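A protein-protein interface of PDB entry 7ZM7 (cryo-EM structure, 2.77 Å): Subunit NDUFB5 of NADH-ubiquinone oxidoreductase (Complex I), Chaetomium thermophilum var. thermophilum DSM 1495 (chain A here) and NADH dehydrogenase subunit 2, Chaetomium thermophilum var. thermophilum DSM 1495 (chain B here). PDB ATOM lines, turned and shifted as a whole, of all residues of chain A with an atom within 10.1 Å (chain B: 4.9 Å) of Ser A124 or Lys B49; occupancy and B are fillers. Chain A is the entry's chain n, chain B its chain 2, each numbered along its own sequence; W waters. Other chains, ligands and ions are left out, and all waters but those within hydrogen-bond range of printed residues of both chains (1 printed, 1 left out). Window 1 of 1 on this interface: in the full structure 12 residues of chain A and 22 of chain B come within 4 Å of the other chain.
The backbone carbonyl oxygen (O) of Lys B49 sits at hydrogen-bond distance from the side-chain hydroxyl (OG1) of Thr B61 (3.2 Å).
NZ of Lys B49 sits at hydrogen-bond distance from O of Ile B567.
NZ of Lys B49 sits at hydrogen-bond distance from O of Leu B568, at 2.5 Å.
The side-chain amino group (NZ) of Lys B49 lies within hydrogen-bond range of the backbone carbonyl oxygen (O) of Ser B570, 3.0 Å away.
The backbone carbonyl oxygen (O) of Leu B568 sits close to the side-chain hydroxyl (OH) of Tyr B296.
O of Ile B567 lies within hydrogen-bond range of OG of Ser B570 (2.6 Å).
Of the 14 printed residues of chain B, 9 touch a printed residue of chain A.
Along chain B the printed residues that touch a printed residue of chain A span positions 49 to 571.
Of the 12 printed residues of chain A, 6 touch a printed residue of chain B.
Printed residues of chain A that touch a printed residue of chain B: Glu A122, Arg A123, Ser A124, Arg A125, Glu A128 and Lys A130.
Among the printed residues, no Asp or Glu carboxylate lies within 4 Å of a Lys or Arg side-chain nitrogen of the other chain.
Water W1 lies within hydrogen-bond range of O of Tyr B296 (2.8 Å), NE of Arg A123 (3.3 Å) and O of Ser A124 (3.4 Å).
The side-chain amino group (NZ) of Lys B49 sits at hydrogen-bond distance from the side-chain hydroxyl (OG) of Ser A124.
The guanidinium group (NH2) of Arg A123 lies close to the backbone carbonyl oxygen (O) of Tyr B296 (3.3 Å).
The side-chain hydroxyl (OH) of Tyr B296 lies within hydrogen-bond range of the side-chain hydroxyl (OG) of Ser A124 (2.6 Å).
The side-chain hydroxyl (OH) of Tyr B297 lies within hydrogen-bond range of the side-chain amino group (NZ) of Lys A130.
N of Ser A124 sits at hydrogen-bond distance from O of Phe B569 (3.4 Å).
O of Ala B571 lies within hydrogen-bond range of N of Ser A124 (3.2 Å).
The backbone carbonyl oxygen of Glu A122 sits close to the backbone carbonyl oxygen of Ala B571 (3.0 Å).
Ser A124 touches just these residues of chain B: Lys B49 (3.4 Å), Tyr B296 (2.6 Å), Phe B569 (3.4 Å), Ser B570 (3.5 Å) and Ala B571 (3.2 Å).
Of chain A, only Ser A124 (3.4 Å), Glu A128 (3.95 Å) and Lys A130 (3.4 Å) come within 4 Å of Lys B49.
No residue of chain A comes within 4 Å of Ser B48.
Of chain A, only Lys A130 comes within 4 Å of Gly B50.
Ser B570 touches just one residue of chain A: Ser A124 (3.5 Å).
Of chain A, only Glu A122, Arg A123 and Ser A124 come within 4 Å of Ala B571.
Printed residues of chain A within 4 Å of Tyr B297: Lys A130.
Of the printed residues of chain A, Ile B51 touches Lys A130.
Of the printed residues of chain B, Glu A122 touches Phe B569 and Ala B571.
Of the printed residues of chain B, Arg A123 touches Tyr B296 (3.2 Å), Asn B301 (3.5 Å), Phe B569 (3.5 Å) and Ala B571 (3.8 Å).
Among the printed residues, pairs that only touch across the chains: Lys A130 with Lys B49 (3.4 Å), Ser A124 with Ser B570 (3.5 Å), Arg A123 with Phe B569 (3.5 Å), Arg A123 with Asn B301 (3.5 Å), Glu A122 with Phe B569 (3.5 Å), Arg A125 with Asn B301 (3.6 Å), Lys A130 with Gly B50 (3.6 Å), Arg A123 with Ala B571 (3.8 Å), Lys A130 with Ile B51 (3.9 Å) and Glu A128 with Lys B49 (3.95 Å).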
ATOM      1  N   THR A 120      -6.142  -8.701  31.878  1.00  0.00           N
ATOM      2  CA  THR A 120      -5.662 -10.059  31.506  1.00  0.00           C
ATOM      3  C   THR A 120      -6.877 -10.837  31.027  1.00  0.00           C
ATOM      4  O   THR A 120      -6.900 -12.058  31.234  1.00  0.00           O
ATOM      5  CB  THR A 120      -4.867 -10.780  32.603  1.00  0.00           C
ATOM      6  OG1 THR A 120      -5.730 -11.108  33.689  1.00  0.00           O
ATOM      7  CG2 THR A 120      -3.647 -10.021  33.078  1.00  0.00           C
ATOM      8  N   ALA A 121      -7.817 -10.162  30.384  1.00  0.00           N
ATOM      9  CA  ALA A 121      -9.081 -10.818  30.011  1.00  0.00           C
ATOM     10  C   ALA A 121      -8.918 -11.560  28.689  1.00  0.00           C
ATOM     11  O   ALA A 121      -7.997 -11.238  27.942  1.00  0.00           O
ATOM     12  CB  ALA A 121     -10.195  -9.807  30.005  1.00  0.00           C
ATOM     13  N   GLU A 122      -9.778 -12.549  28.443  1.00  0.00           N
ATOM     14  CA  GLU A 122      -9.641 -13.367  27.215  1.00  0.00           C
ATOM     15  C   GLU A 122     -10.048 -12.530  25.998  1.00  0.00           C
ATOM     16  O   GLU A 122     -11.133 -11.964  26.008  1.00  0.00           O
ATOM     17  CB  GLU A 122     -10.437 -14.666  27.348  1.00  0.00           C
ATOM     18  CG  GLU A 122     -10.472 -15.494  26.078  1.00  0.00           C
ATOM     19  CD  GLU A 122      -9.129 -16.037  25.621  1.00  0.00           C
ATOM     20  OE1 GLU A 122      -8.274 -16.307  26.487  1.00  0.00           O
ATOM     21  OE2 GLU A 122      -8.940 -16.184  24.396  1.00  0.00           O
ATOM     22  N   ARG A 123      -9.191 -12.484  24.989  1.00  0.00           N
ATOM     23  CA  ARG A 123      -9.503 -11.751  23.743  1.00  0.00           C
ATOM     24  C   ARG A 123     -10.512 -12.574  22.959  1.00  0.00           C
ATOM     25  O   ARG A 123     -10.298 -13.791  22.830  1.00  0.00           O
ATOM     26  CB  ARG A 123      -8.243 -11.620  22.881  1.00  0.00           C
ATOM     27  CG  ARG A 123      -8.374 -10.690  21.687  1.00  0.00           C
ATOM     28  CD  ARG A 123      -7.228 -10.917  20.725  1.00  0.00           C
ATOM     29  NE  ARG A 123      -7.076  -9.844  19.754  1.00  0.00           N
ATOM     30  CZ  ARG A 123      -6.175  -8.876  19.847  1.00  0.00           C
ATOM     31  NH1 ARG A 123      -5.329  -8.850  20.862  1.00  0.00           N
ATOM     32  NH2 ARG A 123      -6.109  -7.946  18.916  1.00  0.00           N
ATOM     33  N   SER A 124     -11.578 -11.938  22.494  1.00  0.00           N
ATOM     34  CA  SER A 124     -12.564 -12.620  21.618  1.00  0.00           C
ATOM     35  C   SER A 124     -11.907 -13.182  20.371  1.00  0.00           C
ATOM     36  O   SER A 124     -11.177 -12.454  19.691  1.00  0.00           O
ATOM     37  CB  SER A 124     -13.651 -11.690  21.217  1.00  0.00           C
ATOM     38  OG  SER A 124     -13.155 -10.672  20.365  1.00  0.00           O
ATOM     39  N   ARG A 125     -12.120 -14.471  20.142  1.00  0.00           N
ATOM     40  CA  ARG A 125     -11.611 -15.116  18.915  1.00  0.00           C
ATOM     41  C   ARG A 125     -12.841 -15.338  18.042  1.00  0.00           C
ATOM     42  O   ARG A 125     -12.683 -15.809  16.904  1.00  0.00           O
ATOM     43  CB  ARG A 125     -10.923 -16.430  19.293  1.00  0.00           C
ATOM     44  CG  ARG A 125      -9.961 -16.310  20.465  1.00  0.00           C
ATOM     45  CD  ARG A 125      -9.352 -17.652  20.811  1.00  0.00           C
ATOM     46  NE  ARG A 125      -8.660 -18.237  19.672  1.00  0.00           N
ATOM     47  CZ  ARG A 125      -8.051 -19.417  19.687  1.00  0.00           C
ATOM     48  NH1 ARG A 125      -8.050 -20.145  20.790  1.00  0.00           N
ATOM     49  NH2 ARG A 125      -7.447 -19.863  18.600  1.00  0.00           N
ATOM     50  N   HIS A 126     -14.013 -14.977  18.567  1.00  0.00           N
ATOM     51  CA  HIS A 126     -15.277 -15.130  17.814  1.00  0.00           C
ATOM     52  C   HIS A 126     -15.710 -13.775  17.261  1.00  0.00           C
ATOM     53  O   HIS A 126     -15.613 -12.785  17.987  1.00  0.00           O
ATOM     54  CB  HIS A 126     -16.357 -15.727  18.709  1.00  0.00           C
ATOM     55  CG  HIS A 126     -17.712 -15.724  18.090  1.00  0.00           C
ATOM     56  ND1 HIS A 126     -17.976 -16.364  16.901  1.00  0.00           N
ATOM     57  CD2 HIS A 126     -18.872 -15.162  18.486  1.00  0.00           C
ATOM     58  CE1 HIS A 126     -19.241 -16.192  16.585  1.00  0.00           C
ATOM     59  NE2 HIS A 126     -19.813 -15.468  17.547  1.00  0.00           N
ATOM     60  N   ILE A 127     -16.179 -13.748  16.020  1.00  0.00           N
ATOM     61  CA  ILE A 127     -16.655 -12.479  15.410  1.00  0.00           C
ATOM     62  C   ILE A 127     -18.177 -12.513  15.364  1.00  0.00           C
ATOM     63  O   ILE A 127     -18.721 -13.527  14.929  1.00  0.00           O
ATOM     64  CB  ILE A 127     -16.025 -12.305  14.013  1.00  0.00           C
ATOM     65  CG1 ILE A 127     -14.518 -12.077  14.128  1.00  0.00           C
ATOM     66  CG2 ILE A 127     -16.702 -11.191  13.232  1.00  0.00           C
ATOM     67  CD1 ILE A 127     -13.743 -12.545  12.937  1.00  0.00           C
ATOM     68  N   GLU A 128     -18.825 -11.451  15.828  1.00  0.00           N
ATOM     69  CA  GLU A 128     -20.300 -11.354  15.728  1.00  0.00           C
ATOM     70  C   GLU A 128     -20.571 -10.364  14.602  1.00  0.00           C
ATOM     71  O   GLU A 128     -19.994  -9.267  14.617  1.00  0.00           O
ATOM     72  CB  GLU A 128     -20.948 -10.973  17.063  1.00  0.00           C
ATOM     73  CG  GLU A 128     -20.555  -9.608  17.592  1.00  0.00           C
ATOM     74  CD  GLU A 128     -21.048  -9.287  18.993  1.00  0.00           C
ATOM     75  OE1 GLU A 128     -21.613 -10.191  19.640  1.00  0.00           O
ATOM     76  OE2 GLU A 128     -20.867  -8.133  19.432  1.00  0.00           O
ATOM     77  N   LEU A 129     -21.378 -10.764  13.631  1.00  0.00           N
ATOM     78  CA  LEU A 129     -21.608  -9.888  12.470  1.00  0.00           C
ATOM     79  C   LEU A 129     -22.284  -8.608  12.950  1.00  0.00           C
ATOM     80  O   LEU A 129     -23.274  -8.716  13.681  1.00  0.00           O
ATOM     81  CB  LEU A 129     -22.467 -10.657  11.461  1.00  0.00           C
ATOM     82  CG  LEU A 129     -21.758 -11.787  10.725  1.00  0.00           C
ATOM     83  CD1 LEU A 129     -22.750 -12.588   9.901  1.00  0.00           C
ATOM     84  CD2 LEU A 129     -20.657 -11.229   9.840  1.00  0.00           C
ATOM     85  N   LYS A 130     -21.765  -7.451  12.536  1.00  0.00           N
ATOM     86  CA  LYS A 130     -22.373  -6.144  12.879  1.00  0.00           C
ATOM     87  C   LYS A 130     -23.599  -6.005  11.987  1.00  0.00           C
ATOM     88  O   LYS A 130     -24.560  -5.345  12.398  1.00  0.00           O
ATOM     89  CB  LYS A 130     -21.352  -5.046  12.574  1.00  0.00           C
ATOM     90  CG  LYS A 130     -20.078  -5.087  13.403  1.00  0.00           C
ATOM     91  CD  LYS A 130     -19.075  -4.041  12.988  1.00  0.00           C
ATOM     92  CE  LYS A 130     -17.871  -3.985  13.901  1.00  0.00           C
ATOM     93  NZ  LYS A 130     -17.348  -5.335  14.217  1.00  0.00           N
ATOM     94  N   TYR A 131     -23.553  -6.628  10.811  1.00  0.00           N
ATOM     95  CA  TYR A 131     -24.691  -6.622   9.861  1.00  0.00           C
ATOM     96  C   TYR A 131     -25.175  -8.062   9.584  1.00  0.00           C
ATOM     97  O   TYR A 131     -24.912  -8.555   8.488  1.00  0.00           O
ATOM     98  CB  TYR A 131     -24.283  -5.803   8.636  1.00  0.00           C
ATOM     99  CG  TYR A 131     -25.312  -5.557   7.569  1.00  0.00           C
ATOM    100  CD1 TYR A 131     -26.399  -4.735   7.797  1.00  0.00           C
ATOM    101  CD2 TYR A 131     -25.148  -6.090   6.304  1.00  0.00           C
ATOM    102  CE1 TYR A 131     -27.329  -4.490   6.803  1.00  0.00           C
ATOM    103  CE2 TYR A 131     -26.067  -5.855   5.301  1.00  0.00           C
ATOM    104  CZ  TYR A 131     -27.160  -5.053   5.553  1.00  0.00           C
ATOM    105  OH  TYR A 131     -28.057  -4.813   4.560  1.00  0.00           O
ATOM    106  N   ILE B  47     -24.290  -0.983  24.178  1.00  0.00           N
ATOM    107  CA  ILE B  47     -23.030  -1.701  24.163  1.00  0.00           C
ATOM    108  C   ILE B  47     -23.026  -2.593  22.935  1.00  0.00           C
ATOM    109  O   ILE B  47     -23.991  -3.326  22.684  1.00  0.00           O
ATOM    110  CB  ILE B  47     -22.827  -2.523  25.436  1.00  0.00           C
ATOM    111  CG1 ILE B  47     -22.859  -1.607  26.646  1.00  0.00           C
ATOM    112  CG2 ILE B  47     -21.550  -3.322  25.354  1.00  0.00           C
ATOM    113  CD1 ILE B  47     -21.790  -0.561  26.643  1.00  0.00           C
ATOM    114  N   SER B  48     -21.954  -2.518  22.166  1.00  0.00           N
ATOM    115  CA  SER B  48     -21.801  -3.333  20.977  1.00  0.00           C
ATOM    116  C   SER B  48     -20.399  -3.134  20.461  1.00  0.00           C
ATOM    117  O   SER B  48     -19.870  -2.023  20.509  1.00  0.00           O
ATOM    118  CB  SER B  48     -22.816  -2.951  19.894  1.00  0.00           C
ATOM    119  OG  SER B  48     -22.666  -1.600  19.510  1.00  0.00           O
ATOM    120  N   LYS B  49     -19.812  -4.211  19.961  1.00  0.00           N
ATOM    121  CA  LYS B  49     -18.619  -4.072  19.149  1.00  0.00           C
ATOM    122  C   LYS B  49     -18.932  -3.371  17.835  1.00  0.00           C
ATOM    123  O   LYS B  49     -18.017  -2.938  17.131  1.00  0.00           O
ATOM    124  CB  LYS B  49     -18.023  -5.441  18.899  1.00  0.00           C
ATOM    125  CG  LYS B  49     -17.393  -6.065  20.110  1.00  0.00           C
ATOM    126  CD  LYS B  49     -16.825  -7.403  19.741  1.00  0.00           C
ATOM    127  CE  LYS B  49     -16.274  -8.143  20.917  1.00  0.00           C
ATOM    128  NZ  LYS B  49     -14.840  -7.880  21.143  1.00  0.00           N
ATOM    129  N   GLY B  50     -20.208  -3.252  17.485  1.00  0.00           N
ATOM    130  CA  GLY B  50     -20.560  -2.550  16.278  1.00  0.00           C
ATOM    131  C   GLY B  50     -21.927  -2.877  15.736  1.00  0.00           C
ATOM    132  O   GLY B  50     -22.433  -3.982  15.925  1.00  0.00           O
ATOM    133  N   ILE B  51     -22.545  -1.902  15.077  1.00  0.00           N
ATOM    134  CA  ILE B  51     -23.820  -2.084  14.398  1.00  0.00           C
ATOM    135  C   ILE B  51     -23.663  -1.584  12.974  1.00  0.00           C
ATOM    136  O   ILE B  51     -23.432  -0.393  12.757  1.00  0.00           O
ATOM    137  CB  ILE B  51     -24.953  -1.337  15.113  1.00  0.00           C
ATOM    138  CG1 ILE B  51     -24.846  -1.535  16.616  1.00  0.00           C
ATOM    139  CG2 ILE B  51     -26.288  -1.792  14.594  1.00  0.00           C
ATOM    140  CD1 ILE B  51     -25.715  -0.646  17.386  1.00  0.00           C
ATOM    141  N   THR B  61     -20.081   2.331  16.560  1.00  0.00           N
ATOM    142  CA  THR B  61     -19.406   1.720  17.694  1.00  0.00           C
ATOM    143  C   THR B  61     -19.331   2.778  18.779  1.00  0.00           C
ATOM    144  O   THR B  61     -19.399   3.973  18.497  1.00  0.00           O
ATOM    145  CB  THR B  61     -18.001   1.201  17.288  1.00  0.00           C
ATOM    146  OG1 THR B  61     -18.119   0.164  16.307  1.00  0.00           O
ATOM    147  CG2 THR B  61     -17.228   0.662  18.444  1.00  0.00           C
ATOM    148  N   TYR B 296      -7.135  -5.270  15.534  1.00  0.00           N
ATOM    149  CA  TYR B 296      -7.759  -6.202  16.498  1.00  0.00           C
ATOM    150  C   TYR B 296      -8.273  -7.472  15.819  1.00  0.00           C
ATOM    151  O   TYR B 296      -8.066  -8.557  16.373  1.00  0.00           O
ATOM    152  CB  TYR B 296      -8.894  -5.535  17.285  1.00  0.00           C
ATOM    153  CG  TYR B 296      -9.542  -6.454  18.286  1.00  0.00           C
ATOM    154  CD1 TYR B 296      -8.987  -6.629  19.539  1.00  0.00           C
ATOM    155  CD2 TYR B 296     -10.677  -7.180  17.971  1.00  0.00           C
ATOM    156  CE1 TYR B 296      -9.545  -7.494  20.459  1.00  0.00           C
ATOM    157  CE2 TYR B 296     -11.246  -8.054  18.880  1.00  0.00           C
ATOM    158  CZ  TYR B 296     -10.674  -8.210  20.130  1.00  0.00           C
ATOM    159  OH  TYR B 296     -11.219  -9.052  21.050  1.00  0.00           O
ATOM    160  N   TYR B 297      -8.920  -7.355  14.665  1.00  0.00           N
ATOM    161  CA  TYR B 297      -9.560  -8.541  14.034  1.00  0.00           C
ATOM    162  C   TYR B 297      -8.621  -9.251  13.064  1.00  0.00           C
ATOM    163  O   TYR B 297      -9.034 -10.283  12.534  1.00  0.00           O
ATOM    164  CB  TYR B 297     -10.858  -8.161  13.331  1.00  0.00           C
ATOM    165  CG  TYR B 297     -11.951  -7.605  14.204  1.00  0.00           C
ATOM    166  CD1 TYR B 297     -12.757  -8.439  14.957  1.00  0.00           C
ATOM    167  CD2 TYR B 297     -12.207  -6.245  14.246  1.00  0.00           C
ATOM    168  CE1 TYR B 297     -13.773  -7.934  15.751  1.00  0.00           C
ATOM    169  CE2 TYR B 297     -13.217  -5.722  15.035  1.00  0.00           C
ATOM    170  CZ  TYR B 297     -14.004  -6.571  15.790  1.00  0.00           C
ATOM    171  OH  TYR B 297     -15.002  -6.069  16.572  1.00  0.00           O
ATOM    172  N   ASN B 301      -4.387 -15.312  17.059  1.00  0.00           N
ATOM    173  CA  ASN B 301      -4.419 -15.881  18.431  1.00  0.00           C
ATOM    174  C   ASN B 301      -3.557 -17.143  18.446  1.00  0.00           C
ATOM    175  O   ASN B 301      -2.807 -17.336  19.421  1.00  0.00           O
ATOM    176  CB  ASN B 301      -5.852 -16.179  18.882  1.00  0.00           C
ATOM    177  CG  ASN B 301      -6.776 -14.986  18.760  1.00  0.00           C
ATOM    178  OD1 ASN B 301      -6.981 -14.251  19.725  1.00  0.00           O
ATOM    179  ND2 ASN B 301      -7.344 -14.784  17.582  1.00  0.00           N
ATOM    180  N   ILE B 567     -14.935  -3.379  25.793  1.00  0.00           N
ATOM    181  CA  ILE B 567     -15.974  -3.823  24.824  1.00  0.00           C
ATOM    182  C   ILE B 567     -15.269  -4.388  23.591  1.00  0.00           C
ATOM    183  O   ILE B 567     -15.613  -5.493  23.174  1.00  0.00           O
ATOM    184  CB  ILE B 567     -16.937  -2.673  24.469  1.00  0.00           C
ATOM    185  CG1 ILE B 567     -17.651  -2.133  25.710  1.00  0.00           C
ATOM    186  CG2 ILE B 567     -17.919  -3.089  23.389  1.00  0.00           C
ATOM    187  CD1 ILE B 567     -18.290  -0.781  25.517  1.00  0.00           C
ATOM    188  N   LEU B 568     -14.316  -3.666  23.015  1.00  0.00           N
ATOM    189  CA  LEU B 568     -13.592  -4.141  21.809  1.00  0.00           C
ATOM    190  C   LEU B 568     -13.006  -5.527  22.059  1.00  0.00           C
ATOM    191  O   LEU B 568     -12.914  -6.272  21.099  1.00  0.00           O
ATOM    192  CB  LEU B 568     -12.486  -3.145  21.445  1.00  0.00           C
ATOM    193  CG  LEU B 568     -11.481  -3.639  20.406  1.00  0.00           C
ATOM    194  CD1 LEU B 568     -12.172  -3.960  19.092  1.00  0.00           C
ATOM    195  CD2 LEU B 568     -10.368  -2.629  20.195  1.00  0.00           C
ATOM    196  N   PHE B 569     -12.557  -5.822  23.279  1.00  0.00           N
ATOM    197  CA  PHE B 569     -11.923  -7.125  23.623  1.00  0.00           C
ATOM    198  C   PHE B 569     -12.932  -8.069  24.271  1.00  0.00           C
ATOM    199  O   PHE B 569     -12.613  -9.251  24.358  1.00  0.00           O
ATOM    200  CB  PHE B 569     -10.757  -6.890  24.582  1.00  0.00           C
ATOM    201  CG  PHE B 569      -9.441  -6.561  23.925  1.00  0.00           C
ATOM    202  CD1 PHE B 569      -9.215  -5.314  23.368  1.00  0.00           C
ATOM    203  CD2 PHE B 569      -8.420  -7.497  23.876  1.00  0.00           C
ATOM    204  CE1 PHE B 569      -8.007  -5.014  22.762  1.00  0.00           C
ATOM    205  CE2 PHE B 569      -7.210  -7.194  23.273  1.00  0.00           C
ATOM    206  CZ  PHE B 569      -7.007  -5.956  22.715  1.00  0.00           C
ATOM    207  N   SER B 570     -14.141  -7.598  24.581  1.00  0.00           N
ATOM    208  CA  SER B 570     -15.157  -8.377  25.339  1.00  0.00           C
ATOM    209  C   SER B 570     -15.543  -9.659  24.625  1.00  0.00           C
ATOM    210  O   SER B 570     -15.467  -9.687  23.392  1.00  0.00           O
ATOM    211  CB  SER B 570     -16.384  -7.577  25.554  1.00  0.00           C
ATOM    212  OG  SER B 570     -17.060  -7.366  24.325  1.00  0.00           O
ATOM    213  N   ALA B 571     -15.936 -10.677  25.398  1.00  0.00           N
ATOM    214  CA  ALA B 571     -16.227 -11.999  24.815  1.00  0.00           C
ATOM    215  C   ALA B 571     -14.938 -12.466  24.146  1.00  0.00           C
ATOM    216  O   ALA B 571     -13.885 -12.235  24.761  1.00  0.00           O
ATOM    217  CB  ALA B 571     -17.395 -11.938  23.858  1.00  0.00           C
HETATM  218  O   HOH W   1      -9.114 -10.957  17.401  1.00  0.00           O
